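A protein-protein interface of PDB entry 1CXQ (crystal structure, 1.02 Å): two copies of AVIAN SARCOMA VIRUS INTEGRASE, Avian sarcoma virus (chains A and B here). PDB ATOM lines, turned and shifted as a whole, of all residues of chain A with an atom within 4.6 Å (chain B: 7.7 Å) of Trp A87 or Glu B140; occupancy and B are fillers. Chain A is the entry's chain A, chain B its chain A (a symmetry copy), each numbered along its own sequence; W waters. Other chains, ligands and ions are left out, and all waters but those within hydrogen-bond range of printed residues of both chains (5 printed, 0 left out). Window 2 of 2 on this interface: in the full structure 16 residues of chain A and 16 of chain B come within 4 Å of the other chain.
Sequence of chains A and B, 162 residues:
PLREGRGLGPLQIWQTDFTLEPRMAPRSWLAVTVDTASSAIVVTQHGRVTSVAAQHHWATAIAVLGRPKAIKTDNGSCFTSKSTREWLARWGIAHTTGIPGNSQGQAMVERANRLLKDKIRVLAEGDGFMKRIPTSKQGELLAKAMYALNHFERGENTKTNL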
ATOM      1  N   GLN A  55       2.435 -23.868 -11.665  1.00  0.00           N
ATOM      2  CA  GLN A  55       1.188 -24.292 -11.022  1.00  0.00           C
ATOM      3  C   GLN A  55       0.301 -23.121 -10.722  1.00  0.00           C
ATOM      4  O   GLN A  55      -0.919 -23.140 -10.968  1.00  0.00           O
ATOM      5  CB  GLN A  55       1.518 -25.103  -9.771  1.00  0.00           C
ATOM      6  CG  GLN A  55       2.289 -26.398 -10.114  1.00  0.00           C
ATOM      7  CD  GLN A  55       3.036 -26.970  -8.917  1.00  0.00           C
ATOM      8  OE1 GLN A  55       2.638 -26.777  -7.764  1.00  0.00           O
ATOM      9  NE2 GLN A  55       4.104 -27.691  -9.161  1.00  0.00           N
ATOM     10  N   HIS A  56       0.881 -22.031 -10.176  1.00  0.00           N
ATOM     11  CA  HIS A  56       0.085 -20.828  -9.955  1.00  0.00           C
ATOM     12  C   HIS A  56      -0.504 -20.306 -11.231  1.00  0.00           C
ATOM     13  O   HIS A  56      -1.669 -19.864 -11.276  1.00  0.00           O
ATOM     14  CB  HIS A  56       0.944 -19.755  -9.308  1.00  0.00           C
ATOM     15  CG  HIS A  56       1.340 -20.000  -7.882  1.00  0.00           C
ATOM     16  ND1 HIS A  56       0.885 -21.039  -7.093  1.00  0.00           N
ATOM     17  CD2 HIS A  56       2.153 -19.270  -7.081  1.00  0.00           C
ATOM     18  CE1 HIS A  56       1.393 -20.939  -5.860  1.00  0.00           C
ATOM     19  NE2 HIS A  56       2.148 -19.886  -5.837  1.00  0.00           N
ATOM     20  N   TRP A  58      -1.179 -22.030 -14.045  1.00  0.00           N
ATOM     21  CA  TRP A  58      -2.269 -22.896 -14.527  1.00  0.00           C
ATOM     22  C   TRP A  58      -3.497 -22.751 -13.676  1.00  0.00           C
ATOM     23  O   TRP A  58      -4.615 -22.866 -14.206  1.00  0.00           O
ATOM     24  CB  TRP A  58      -1.802 -24.360 -14.592  1.00  0.00           C
ATOM     25  CG  TRP A  58      -0.949 -24.697 -15.763  1.00  0.00           C
ATOM     26  CD1 TRP A  58      -1.042 -24.235 -17.045  1.00  0.00           C
ATOM     27  CD2 TRP A  58       0.144 -25.628 -15.757  1.00  0.00           C
ATOM     28  NE1 TRP A  58      -0.094 -24.815 -17.835  1.00  0.00           N
ATOM     29  CE2 TRP A  58       0.657 -25.673 -17.068  1.00  0.00           C
ATOM     30  CE3 TRP A  58       0.702 -26.414 -14.754  1.00  0.00           C
ATOM     31  CZ2 TRP A  58       1.723 -26.480 -17.390  1.00  0.00           C
ATOM     32  CZ3 TRP A  58       1.770 -27.223 -15.101  1.00  0.00           C
ATOM     33  CH2 TRP A  58       2.268 -27.250 -16.396  1.00  0.00           C
ATOM     34  N   ALA A  59      -3.362 -22.538 -12.367  1.00  0.00           N
ATOM     35  CA  ALA A  59      -4.551 -22.336 -11.549  1.00  0.00           C
ATOM     36  C   ALA A  59      -5.364 -21.168 -12.113  1.00  0.00           C
ATOM     37  O   ALA A  59      -6.595 -21.221 -12.237  1.00  0.00           O
ATOM     38  CB  ALA A  59      -4.160 -22.096 -10.107  1.00  0.00           C
ATOM     39  N   ILE A  62      -6.953 -22.064 -15.535  1.00  0.00           N
ATOM     40  CA  ILE A  62      -8.159 -22.889 -15.370  1.00  0.00           C
ATOM     41  C   ILE A  62      -9.352 -22.016 -14.993  1.00  0.00           C
ATOM     42  O   ILE A  62     -10.461 -22.224 -15.491  1.00  0.00           O
ATOM     43  CB  ILE A  62      -7.907 -24.000 -14.342  1.00  0.00           C
ATOM     44  CG1 ILE A  62      -6.887 -25.023 -14.860  1.00  0.00           C
ATOM     45  CG2 ILE A  62      -9.172 -24.683 -13.926  1.00  0.00           C
ATOM     46  CD1 ILE A  62      -6.351 -25.931 -13.768  1.00  0.00           C
ATOM     47  N   SER A  83       6.772 -32.416  -8.458  1.00  0.00           N
ATOM     48  CA  SER A  83       5.764 -31.507  -7.969  1.00  0.00           C
ATOM     49  C   SER A  83       4.731 -31.169  -9.046  1.00  0.00           C
ATOM     50  O   SER A  83       3.516 -31.244  -8.812  1.00  0.00           O
ATOM     51  CB  SER A  83       6.455 -30.200  -7.479  1.00  0.00           C
ATOM     52  OG  SER A  83       5.579 -29.234  -7.183  1.00  0.00           O
ATOM     53  N   THR A  84       5.228 -30.786 -10.212  1.00  0.00           N
ATOM     54  CA  THR A  84       4.294 -30.434 -11.296  1.00  0.00           C
ATOM     55  C   THR A  84       3.517 -31.619 -11.774  1.00  0.00           C
ATOM     56  O   THR A  84       2.299 -31.513 -12.050  1.00  0.00           O
ATOM     57  CB  THR A  84       5.046 -29.694 -12.399  1.00  0.00           C
ATOM     58  OG1 THR A  84       5.469 -28.446 -11.799  1.00  0.00           O
ATOM     59  CG2 THR A  84       4.122 -29.518 -13.591  1.00  0.00           C
ATOM     60  N   ARG A  85       4.183 -32.781 -11.909  1.00  0.00           N
ATOM     61  CA  ARG A  85       3.456 -33.961 -12.313  1.00  0.00           C
ATOM     62  C   ARG A  85       2.327 -34.305 -11.353  1.00  0.00           C
ATOM     63  O   ARG A  85       1.191 -34.649 -11.751  1.00  0.00           O
ATOM     64  CB  ARG A  85       4.458 -35.070 -12.557  1.00  0.00           C
ATOM     65  CG  ARG A  85       5.296 -34.534 -13.806  1.00  0.00           C
ATOM     66  CD  ARG A  85       6.231 -35.598 -14.392  1.00  0.00           C
ATOM     67  NE  ARG A  85       5.456 -36.630 -15.068  1.00  0.00           N
ATOM     68  CZ  ARG A  85       5.923 -37.778 -15.495  1.00  0.00           C
ATOM     69  NH1 ARG A  85       7.212 -38.049 -15.363  1.00  0.00           N
ATOM     70  NH2 ARG A  85       5.083 -38.622 -16.072  1.00  0.00           N
ATOM     71  N   GLU A  86       2.595 -34.170 -10.073  1.00  0.00           N
ATOM     72  CA  GLU A  86       1.570 -34.436  -9.060  1.00  0.00           C
ATOM     73  C   GLU A  86       0.430 -33.411  -9.107  1.00  0.00           C
ATOM     74  O   GLU A  86      -0.743 -33.765  -8.944  1.00  0.00           O
ATOM     75  CB  GLU A  86       2.205 -34.500  -7.677  1.00  0.00           C
ATOM     76  CG  GLU A  86       1.185 -34.607  -6.564  1.00  0.00           C
ATOM     77  CD  GLU A  86       0.242 -35.743  -6.550  1.00  0.00           C
ATOM     78  OE1 GLU A  86       0.389 -36.756  -7.291  1.00  0.00           O
ATOM     79  OE2 GLU A  86      -0.725 -35.658  -5.750  1.00  0.00           O
ATOM     80  N   TRP A  87       0.756 -32.147  -9.330  1.00  0.00           N
ATOM     81  CA  TRP A  87      -0.270 -31.096  -9.405  1.00  0.00           C
ATOM     82  C   TRP A  87      -1.204 -31.343 -10.577  1.00  0.00           C
ATOM     83  O   TRP A  87      -2.422 -31.248 -10.465  1.00  0.00           O
ATOM     84  CB  TRP A  87       0.441 -29.737  -9.504  1.00  0.00           C
ATOM     85  CG  TRP A  87      -0.437 -28.545  -9.401  1.00  0.00           C
ATOM     86  CD1 TRP A  87      -0.634 -27.810  -8.257  1.00  0.00           C
ATOM     87  CD2 TRP A  87      -1.232 -27.922 -10.409  1.00  0.00           C
ATOM     88  NE1 TRP A  87      -1.496 -26.770  -8.489  1.00  0.00           N
ATOM     89  CE2 TRP A  87      -1.889 -26.802  -9.813  1.00  0.00           C
ATOM     90  CE3 TRP A  87      -1.458 -28.154 -11.762  1.00  0.00           C
ATOM     91  CZ2 TRP A  87      -2.731 -25.969 -10.536  1.00  0.00           C
ATOM     92  CZ3 TRP A  87      -2.304 -27.332 -12.467  1.00  0.00           C
ATOM     93  CH2 TRP A  87      -2.936 -26.252 -11.851  1.00  0.00           C
ATOM     94  N   LEU A  88      -0.644 -31.701 -11.732  1.00  0.00           N
ATOM     95  CA  LEU A  88      -1.480 -31.990 -12.894  1.00  0.00           C
ATOM     96  C   LEU A  88      -2.315 -33.240 -12.661  1.00  0.00           C
ATOM     97  O   LEU A  88      -3.486 -33.294 -13.071  1.00  0.00           O
ATOM     98  CB  LEU A  88      -0.616 -32.144 -14.149  1.00  0.00           C
ATOM     99  CG  LEU A  88       0.003 -30.809 -14.639  1.00  0.00           C
ATOM    100  CD1 LEU A  88       1.106 -31.069 -15.641  1.00  0.00           C
ATOM    101  CD2 LEU A  88      -1.079 -29.926 -15.222  1.00  0.00           C
ATOM    102  N   ALA A  89      -1.763 -34.263 -12.001  1.00  0.00           N
ATOM    103  CA  ALA A  89      -2.535 -35.465 -11.689  1.00  0.00           C
ATOM    104  C   ALA A  89      -3.683 -35.140 -10.732  1.00  0.00           C
ATOM    105  O   ALA A  89      -4.786 -35.675 -10.888  1.00  0.00           O
ATOM    106  CB  ALA A  89      -1.626 -36.543 -11.112  1.00  0.00           C
ATOM    107  N   ARG A  90      -3.447 -34.277  -9.765  1.00  0.00           N
ATOM    108  CA  ARG A  90      -4.498 -33.823  -8.831  1.00  0.00           C
ATOM    109  C   ARG A  90      -5.686 -33.233  -9.558  1.00  0.00           C
ATOM    110  O   ARG A  90      -6.834 -33.424  -9.170  1.00  0.00           O
ATOM    111  CB  ARG A  90      -3.864 -32.792  -7.890  1.00  0.00           C
ATOM    112  CG  ARG A  90      -4.824 -32.196  -6.899  1.00  0.00           C
ATOM    113  CD  ARG A  90      -4.363 -30.843  -6.372  1.00  0.00           C
ATOM    114  NE  ARG A  90      -3.002 -30.917  -5.861  1.00  0.00           N
ATOM    115  CZ  ARG A  90      -2.248 -29.867  -5.516  1.00  0.00           C
ATOM    116  NH1 ARG A  90      -2.732 -28.648  -5.615  1.00  0.00           N
ATOM    117  NH2 ARG A  90      -0.993 -30.094  -5.092  1.00  0.00           N
ATOM    118  N   TRP A  91      -5.403 -32.480 -10.623  1.00  0.00           N
ATOM    119  CA  TRP A  91      -6.413 -31.860 -11.457  1.00  0.00           C
ATOM    120  C   TRP A  91      -6.981 -32.788 -12.515  1.00  0.00           C
ATOM    121  O   TRP A  91      -7.968 -32.391 -13.168  1.00  0.00           O
ATOM    122  CB  TRP A  91      -5.842 -30.607 -12.115  1.00  0.00           C
ATOM    123  CG  TRP A  91      -5.916 -29.377 -11.236  1.00  0.00           C
ATOM    124  CD1 TRP A  91      -4.983 -28.831 -10.455  1.00  0.00           C
ATOM    125  CD2 TRP A  91      -7.090 -28.571 -11.126  1.00  0.00           C
ATOM    126  NE1 TRP A  91      -5.478 -27.703  -9.819  1.00  0.00           N
ATOM    127  CE2 TRP A  91      -6.765 -27.530 -10.229  1.00  0.00           C
ATOM    128  CE3 TRP A  91      -8.357 -28.634 -11.680  1.00  0.00           C
ATOM    129  CZ2 TRP A  91      -7.699 -26.545  -9.899  1.00  0.00           C
ATOM    130  CZ3 TRP A  91      -9.281 -27.653 -11.357  1.00  0.00           C
ATOM    131  CH2 TRP A  91      -8.954 -26.633 -10.479  1.00  0.00           C
ATOM    132  N   MET B  24      -9.352 -14.651   3.424  1.00  0.00           N
ATOM    133  CA  MET B  24      -8.367 -14.231   2.443  1.00  0.00           C
ATOM    134  C   MET B  24      -7.448 -13.089   2.933  1.00  0.00           C
ATOM    135  O   MET B  24      -6.701 -12.542   2.150  1.00  0.00           O
ATOM    136  CB  MET B  24      -9.082 -13.832   1.152  1.00  0.00           C
ATOM    137  CG  MET B  24      -9.693 -15.013   0.417  1.00  0.00           C
ATOM    138  SD  MET B  24      -8.430 -15.866  -0.551  1.00  0.00           S
ATOM    139  CE  MET B  24      -9.376 -17.244  -1.139  1.00  0.00           C
ATOM    140  N   GLN B  45      -8.293 -10.333  -5.443  1.00  0.00           N
ATOM    141  CA  GLN B  45      -8.213  -9.924  -4.033  1.00  0.00           C
ATOM    142  C   GLN B  45      -7.254  -8.723  -3.913  1.00  0.00           C
ATOM    143  O   GLN B  45      -6.324  -8.495  -4.687  1.00  0.00           O
ATOM    144  CB  GLN B  45      -7.845 -11.160  -3.136  1.00  0.00           C
ATOM    145  CG  GLN B  45      -6.446 -11.648  -3.403  1.00  0.00           C
ATOM    146  CD  GLN B  45      -6.088 -12.874  -2.568  1.00  0.00           C
ATOM    147  OE1 GLN B  45      -5.583 -13.903  -3.074  1.00  0.00           O
ATOM    148  NE2 GLN B  45      -6.281 -12.830  -1.237  1.00  0.00           N
ATOM    149  N   LEU B 123     -14.018 -24.969   0.026  1.00  0.00           N
ATOM    150  CA  LEU B 123     -12.701 -25.390  -0.471  1.00  0.00           C
ATOM    151  C   LEU B 123     -11.660 -25.322   0.654  1.00  0.00           C
ATOM    152  O   LEU B 123     -10.835 -26.196   0.817  1.00  0.00           O
ATOM    153  CB  LEU B 123     -12.284 -24.578  -1.679  1.00  0.00           C
ATOM    154  CG  LEU B 123     -13.172 -24.726  -2.914  1.00  0.00           C
ATOM    155  CD1 LEU B 123     -12.730 -23.708  -3.978  1.00  0.00           C
ATOM    156  CD2 LEU B 123     -13.199 -26.131  -3.473  1.00  0.00           C
ATOM    157  N   ASP B 127      -9.453 -28.382   2.535  1.00  0.00           N
ATOM    158  CA  ASP B 127      -8.007 -28.398   2.679  1.00  0.00           C
ATOM    159  C   ASP B 127      -7.569 -28.346   4.149  1.00  0.00           C
ATOM    160  O   ASP B 127      -6.371 -28.304   4.425  1.00  0.00           O
ATOM    161  CB  ASP B 127      -7.404 -27.227   1.898  1.00  0.00           C
ATOM    162  CG  ASP B 127      -7.395 -27.392   0.411  1.00  0.00           C
ATOM    163  OD1 ASP B 127      -7.617 -28.532  -0.068  1.00  0.00           O
ATOM    164  OD2 ASP B 127      -7.124 -26.377  -0.268  1.00  0.00           O
ATOM    165  N   THR B 135      -1.471 -17.644   3.594  1.00  0.00           N
ATOM    166  CA  THR B 135      -1.290 -16.707   2.498  1.00  0.00           C
ATOM    167  C   THR B 135      -0.791 -17.382   1.241  1.00  0.00           C
ATOM    168  O   THR B 135      -1.270 -17.058   0.131  1.00  0.00           O
ATOM    169  CB  THR B 135      -0.350 -15.581   2.942  1.00  0.00           C
ATOM    170  OG1 THR B 135      -0.912 -15.025   4.131  1.00  0.00           O
ATOM    171  CG2 THR B 135      -0.296 -14.521   1.848  1.00  0.00           C
ATOM    172  N   SER B 136       0.138 -18.322   1.372  1.00  0.00           N
ATOM    173  CA  SER B 136       0.713 -18.976   0.213  1.00  0.00           C
ATOM    174  C   SER B 136      -0.244 -19.883  -0.547  1.00  0.00           C
ATOM    175  O   SER B 136       0.087 -20.338  -1.639  1.00  0.00           O
ATOM    176  CB  SER B 136       1.932 -19.827   0.668  1.00  0.00           C
ATOM    177  OG  SER B 136       1.531 -20.926   1.454  1.00  0.00           O
ATOM    178  N   LYS B 137      -1.399 -20.160   0.043  1.00  0.00           N
ATOM    179  CA  LYS B 137      -2.396 -21.072  -0.562  1.00  0.00           C
ATOM    180  C   LYS B 137      -3.572 -20.289  -1.152  1.00  0.00           C
ATOM    181  O   LYS B 137      -4.416 -20.885  -1.856  1.00  0.00           O
ATOM    182  CB  LYS B 137      -2.895 -22.071   0.458  1.00  0.00           C
ATOM    183  CG  LYS B 137      -1.803 -22.963   1.023  1.00  0.00           C
ATOM    184  CD  LYS B 137      -1.128 -23.807  -0.030  1.00  0.00           C
ATOM    185  CE  LYS B 137       0.000 -24.631   0.585  1.00  0.00           C
ATOM    186  NZ  LYS B 137       0.518 -25.500  -0.561  1.00  0.00           N
ATOM    187  N   GLN B 138      -3.681 -19.001  -0.889  1.00  0.00           N
ATOM    188  CA  GLN B 138      -4.876 -18.234  -1.233  1.00  0.00           C
ATOM    189  C   GLN B 138      -5.068 -18.070  -2.723  1.00  0.00           C
ATOM    190  O   GLN B 138      -6.205 -18.154  -3.186  1.00  0.00           O
ATOM    191  CB  GLN B 138      -4.794 -16.839  -0.598  1.00  0.00           C
ATOM    192  CG  GLN B 138      -5.041 -16.893   0.915  1.00  0.00           C
ATOM    193  CD  GLN B 138      -4.813 -15.538   1.536  1.00  0.00           C
ATOM    194  OE1 GLN B 138      -4.619 -14.527   0.840  1.00  0.00           O
ATOM    195  NE2 GLN B 138      -4.897 -15.484   2.860  1.00  0.00           N
ATOM    196  N   GLY B 139      -4.015 -17.760  -3.473  1.00  0.00           N
ATOM    197  CA  GLY B 139      -4.226 -17.482  -4.864  1.00  0.00           C
ATOM    198  C   GLY B 139      -4.830 -18.645  -5.614  1.00  0.00           C
ATOM    199  O   GLY B 139      -5.769 -18.494  -6.407  1.00  0.00           O
ATOM    200  N   GLU B 140      -4.271 -19.851  -5.385  1.00  0.00           N
ATOM    201  CA  GLU B 140      -4.828 -21.003  -6.079  1.00  0.00           C
ATOM    202  C   GLU B 140      -6.212 -21.336  -5.566  1.00  0.00           C
ATOM    203  O   GLU B 140      -7.056 -21.811  -6.337  1.00  0.00           O
ATOM    204  CB  GLU B 140      -3.927 -22.236  -5.972  1.00  0.00           C
ATOM    205  CG  GLU B 140      -2.642 -22.109  -6.750  1.00  0.00           C
ATOM    206  CD  GLU B 140      -1.877 -23.375  -6.998  1.00  0.00           C
ATOM    207  OE1 GLU B 140      -2.467 -24.490  -6.936  1.00  0.00           O
ATOM    208  OE2 GLU B 140      -0.692 -23.289  -7.349  1.00  0.00           O
ATOM    209  N   LEU B 141      -6.492 -21.128  -4.277  1.00  0.00           N
ATOM    210  CA  LEU B 141      -7.817 -21.434  -3.764  1.00  0.00           C
ATOM    211  C   LEU B 141      -8.840 -20.478  -4.377  1.00  0.00           C
ATOM    212  O   LEU B 141      -9.938 -20.907  -4.769  1.00  0.00           O
ATOM    213  CB  LEU B 141      -7.836 -21.450  -2.242  1.00  0.00           C
ATOM    214  CG  LEU B 141      -9.077 -22.057  -1.606  1.00  0.00           C
ATOM    215  CD1 LEU B 141      -8.739 -22.661  -0.257  1.00  0.00           C
ATOM    216  CD2 LEU B 141     -10.216 -21.057  -1.488  1.00  0.00           C
ATOM    217  N   LEU B 142      -8.514 -19.202  -4.465  1.00  0.00           N
ATOM    218  CA  LEU B 142      -9.418 -18.228  -5.073  1.00  0.00           C
ATOM    219  C   LEU B 142      -9.685 -18.584  -6.551  1.00  0.00           C
ATOM    220  O   LEU B 142     -10.815 -18.538  -7.023  1.00  0.00           O
ATOM    221  CB  LEU B 142      -8.839 -16.829  -4.940  1.00  0.00           C
ATOM    222  CG  LEU B 142      -9.761 -15.720  -5.420  1.00  0.00           C
ATOM    223  CD1 LEU B 142     -11.007 -15.638  -4.530  1.00  0.00           C
ATOM    224  CD2 LEU B 142      -9.023 -14.388  -5.395  1.00  0.00           C
ATOM    225  N   ALA B 143      -8.605 -18.939  -7.267  1.00  0.00           N
ATOM    226  CA  ALA B 143      -8.772 -19.356  -8.652  1.00  0.00           C
ATOM    227  C   ALA B 143      -9.633 -20.602  -8.758  1.00  0.00           C
ATOM    228  O   ALA B 143     -10.427 -20.736  -9.707  1.00  0.00           O
ATOM    229  CB  ALA B 143      -7.403 -19.604  -9.286  1.00  0.00           C
ATOM    230  N   LYS B 144      -9.498 -21.520  -7.829  1.00  0.00           N
ATOM    231  CA  LYS B 144     -10.330 -22.738  -7.812  1.00  0.00           C
ATOM    232  C   LYS B 144     -11.787 -22.403  -7.604  1.00  0.00           C
ATOM    233  O   LYS B 144     -12.665 -23.000  -8.230  1.00  0.00           O
ATOM    234  CB  LYS B 144      -9.773 -23.695  -6.765  1.00  0.00           C
ATOM    235  CG  LYS B 144     -10.456 -25.057  -6.756  1.00  0.00           C
ATOM    236  CD  LYS B 144      -9.943 -25.957  -5.659  1.00  0.00           C
ATOM    237  CE  LYS B 144      -8.524 -26.361  -5.789  1.00  0.00           C
ATOM    238  NZ  LYS B 144      -8.077 -27.089  -4.548  1.00  0.00           N
ATOM    239  N   ALA B 145     -12.065 -21.442  -6.719  1.00  0.00           N
ATOM    240  CA  ALA B 145     -13.451 -21.010  -6.493  1.00  0.00           C
ATOM    241  C   ALA B 145     -14.026 -20.382  -7.755  1.00  0.00           C
ATOM    242  O   ALA B 145     -15.198 -20.641  -8.100  1.00  0.00           O
ATOM    243  CB  ALA B 145     -13.517 -20.064  -5.324  1.00  0.00           C
ATOM    244  N   MET B 146     -13.254 -19.543  -8.429  1.00  0.00           N
ATOM    245  CA  MET B 146     -13.693 -18.927  -9.647  1.00  0.00           C
ATOM    246  C   MET B 146     -13.977 -19.985 -10.728  1.00  0.00           C
ATOM    247  O   MET B 146     -14.994 -19.952 -11.415  1.00  0.00           O
ATOM    248  CB  MET B 146     -12.655 -17.929 -10.130  1.00  0.00           C
ATOM    249  CG  MET B 146     -13.006 -17.171 -11.401  1.00  0.00           C
ATOM    250  SD  MET B 146     -11.818 -15.875 -11.706  1.00  0.00           S
ATOM    251  CE  MET B 146     -11.978 -15.698 -13.485  1.00  0.00           C
ATOM    252  N   TYR B 147     -13.033 -20.936 -10.887  1.00  0.00           N
ATOM    253  CA  TYR B 147     -13.262 -22.064 -11.779  1.00  0.00           C
ATOM    254  C   TYR B 147     -14.545 -22.792 -11.463  1.00  0.00           C
ATOM    255  O   TYR B 147     -15.351 -23.104 -12.362  1.00  0.00           O
ATOM    256  CB  TYR B 147     -12.062 -23.033 -11.668  1.00  0.00           C
ATOM    257  CG  TYR B 147     -12.395 -24.461 -12.015  1.00  0.00           C
ATOM    258  CD1 TYR B 147     -12.590 -24.900 -13.303  1.00  0.00           C
ATOM    259  CD2 TYR B 147     -12.512 -25.393 -10.999  1.00  0.00           C
ATOM    260  CE1 TYR B 147     -12.907 -26.239 -13.569  1.00  0.00           C
ATOM    261  CE2 TYR B 147     -12.800 -26.725 -11.257  1.00  0.00           C
ATOM    262  CZ  TYR B 147     -12.987 -27.132 -12.542  1.00  0.00           C
ATOM    263  OH  TYR B 147     -13.275 -28.450 -12.854  1.00  0.00           O
HETATM  264  O   HOH W   1      -1.302 -18.482  -6.558  1.00  0.00           O
HETATM  265  O   HOH W   2       2.408 -20.050  -3.023  1.00  0.00           O
HETATM  266  O   HOH W   3      -8.137 -22.994 -10.697  1.00  0.00           O
HETATM  267  O   HOH W   4      -4.902 -25.557  -7.774  1.00  0.00           O
HETATM  268  O   HOH W   5       0.951 -25.186  -6.247  1.00  0.00           O
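No position is printed for both chains.
The side-chain amide nitrogen of Gln A55 sits at hydrogen-bond distance from the side-chain hydroxyl of Ser A83 (2.9 Å). The side-chain hydroxyl of Thr A84 lies within hydrogen-bond range of the side-chain amide nitrogen of Gln A55 (3.1 Å).
Of the 14 printed residues of chain A, 6 touch a printed residue of chain B. Hydrophobic or aromatic side chains of chain A that line the printed part of chain B: His A56, Ala A59, Ile A62, Trp A87 and Trp A91. Of the 17 printed residues of chain B, 3 touch a printed residue of chain A.
Trp A87 touches just one residue of chain B: Glu B140 (2.9 Å). Of chain A, only Gln A55 (3.5 Å), His A56 (2.8 Å), Ala A59 (3.7 Å) and Trp A87 (2.9 Å) come within 4 Å of Glu B140. Of the printed residues of chain A, Tyr B147 touches Ile A62 (3.5 Å) and Trp A91 (3.6 Å). Of the printed residues of chain B, Gln A55 touches Glu B140. Ser A83 touches none of the printed residues of chain B. Arg A85 touches none of the printed residues of chain B. The nearest residue of chain B that does not touch Trp A87 is Lys B144 (7.5 Å). The nearest printed residue of chain A that does not touch Ala B143 is Ile A62 (5.5 Å).
ND1 of His A56 is in hydrogen-bond range of OE2 of Glu B140, at 2.8 Å. NE1 of Trp A87 lies within hydrogen-bond range of OE1 of Glu B140 (2.9 Å).
Among the printed residues, pairs that only touch across the chains: Gln A55 with Glu B140 (3.5 Å), Ala A59 with Glu B140 (3.7 Å), Ala A59 with Ala B143 (3.5 Å), Ile A62 with Tyr B147 (3.5 Å) and Trp A91 with Tyr B147 (3.6 Å).
Water W2 lies within hydrogen-bond range of O of Ser B136 and NE2 of His A56. Water W5 bridges the side-chain carboxylate of Glu B140 (2.7 Å) and the side-chain amide oxygen of Gln A55 (2.8 Å). Water W4 lies within hydrogen-bond range of OE1 of Glu B140 (2.8 Å) and NE1 of Trp A91 (3.0 Å). Water W3 bridges O of Ala A59 (2.8 Å) and O of Ala B143 (3.4 Å). Water W1 bridges ND1 of His A56 and N of Glu B140.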
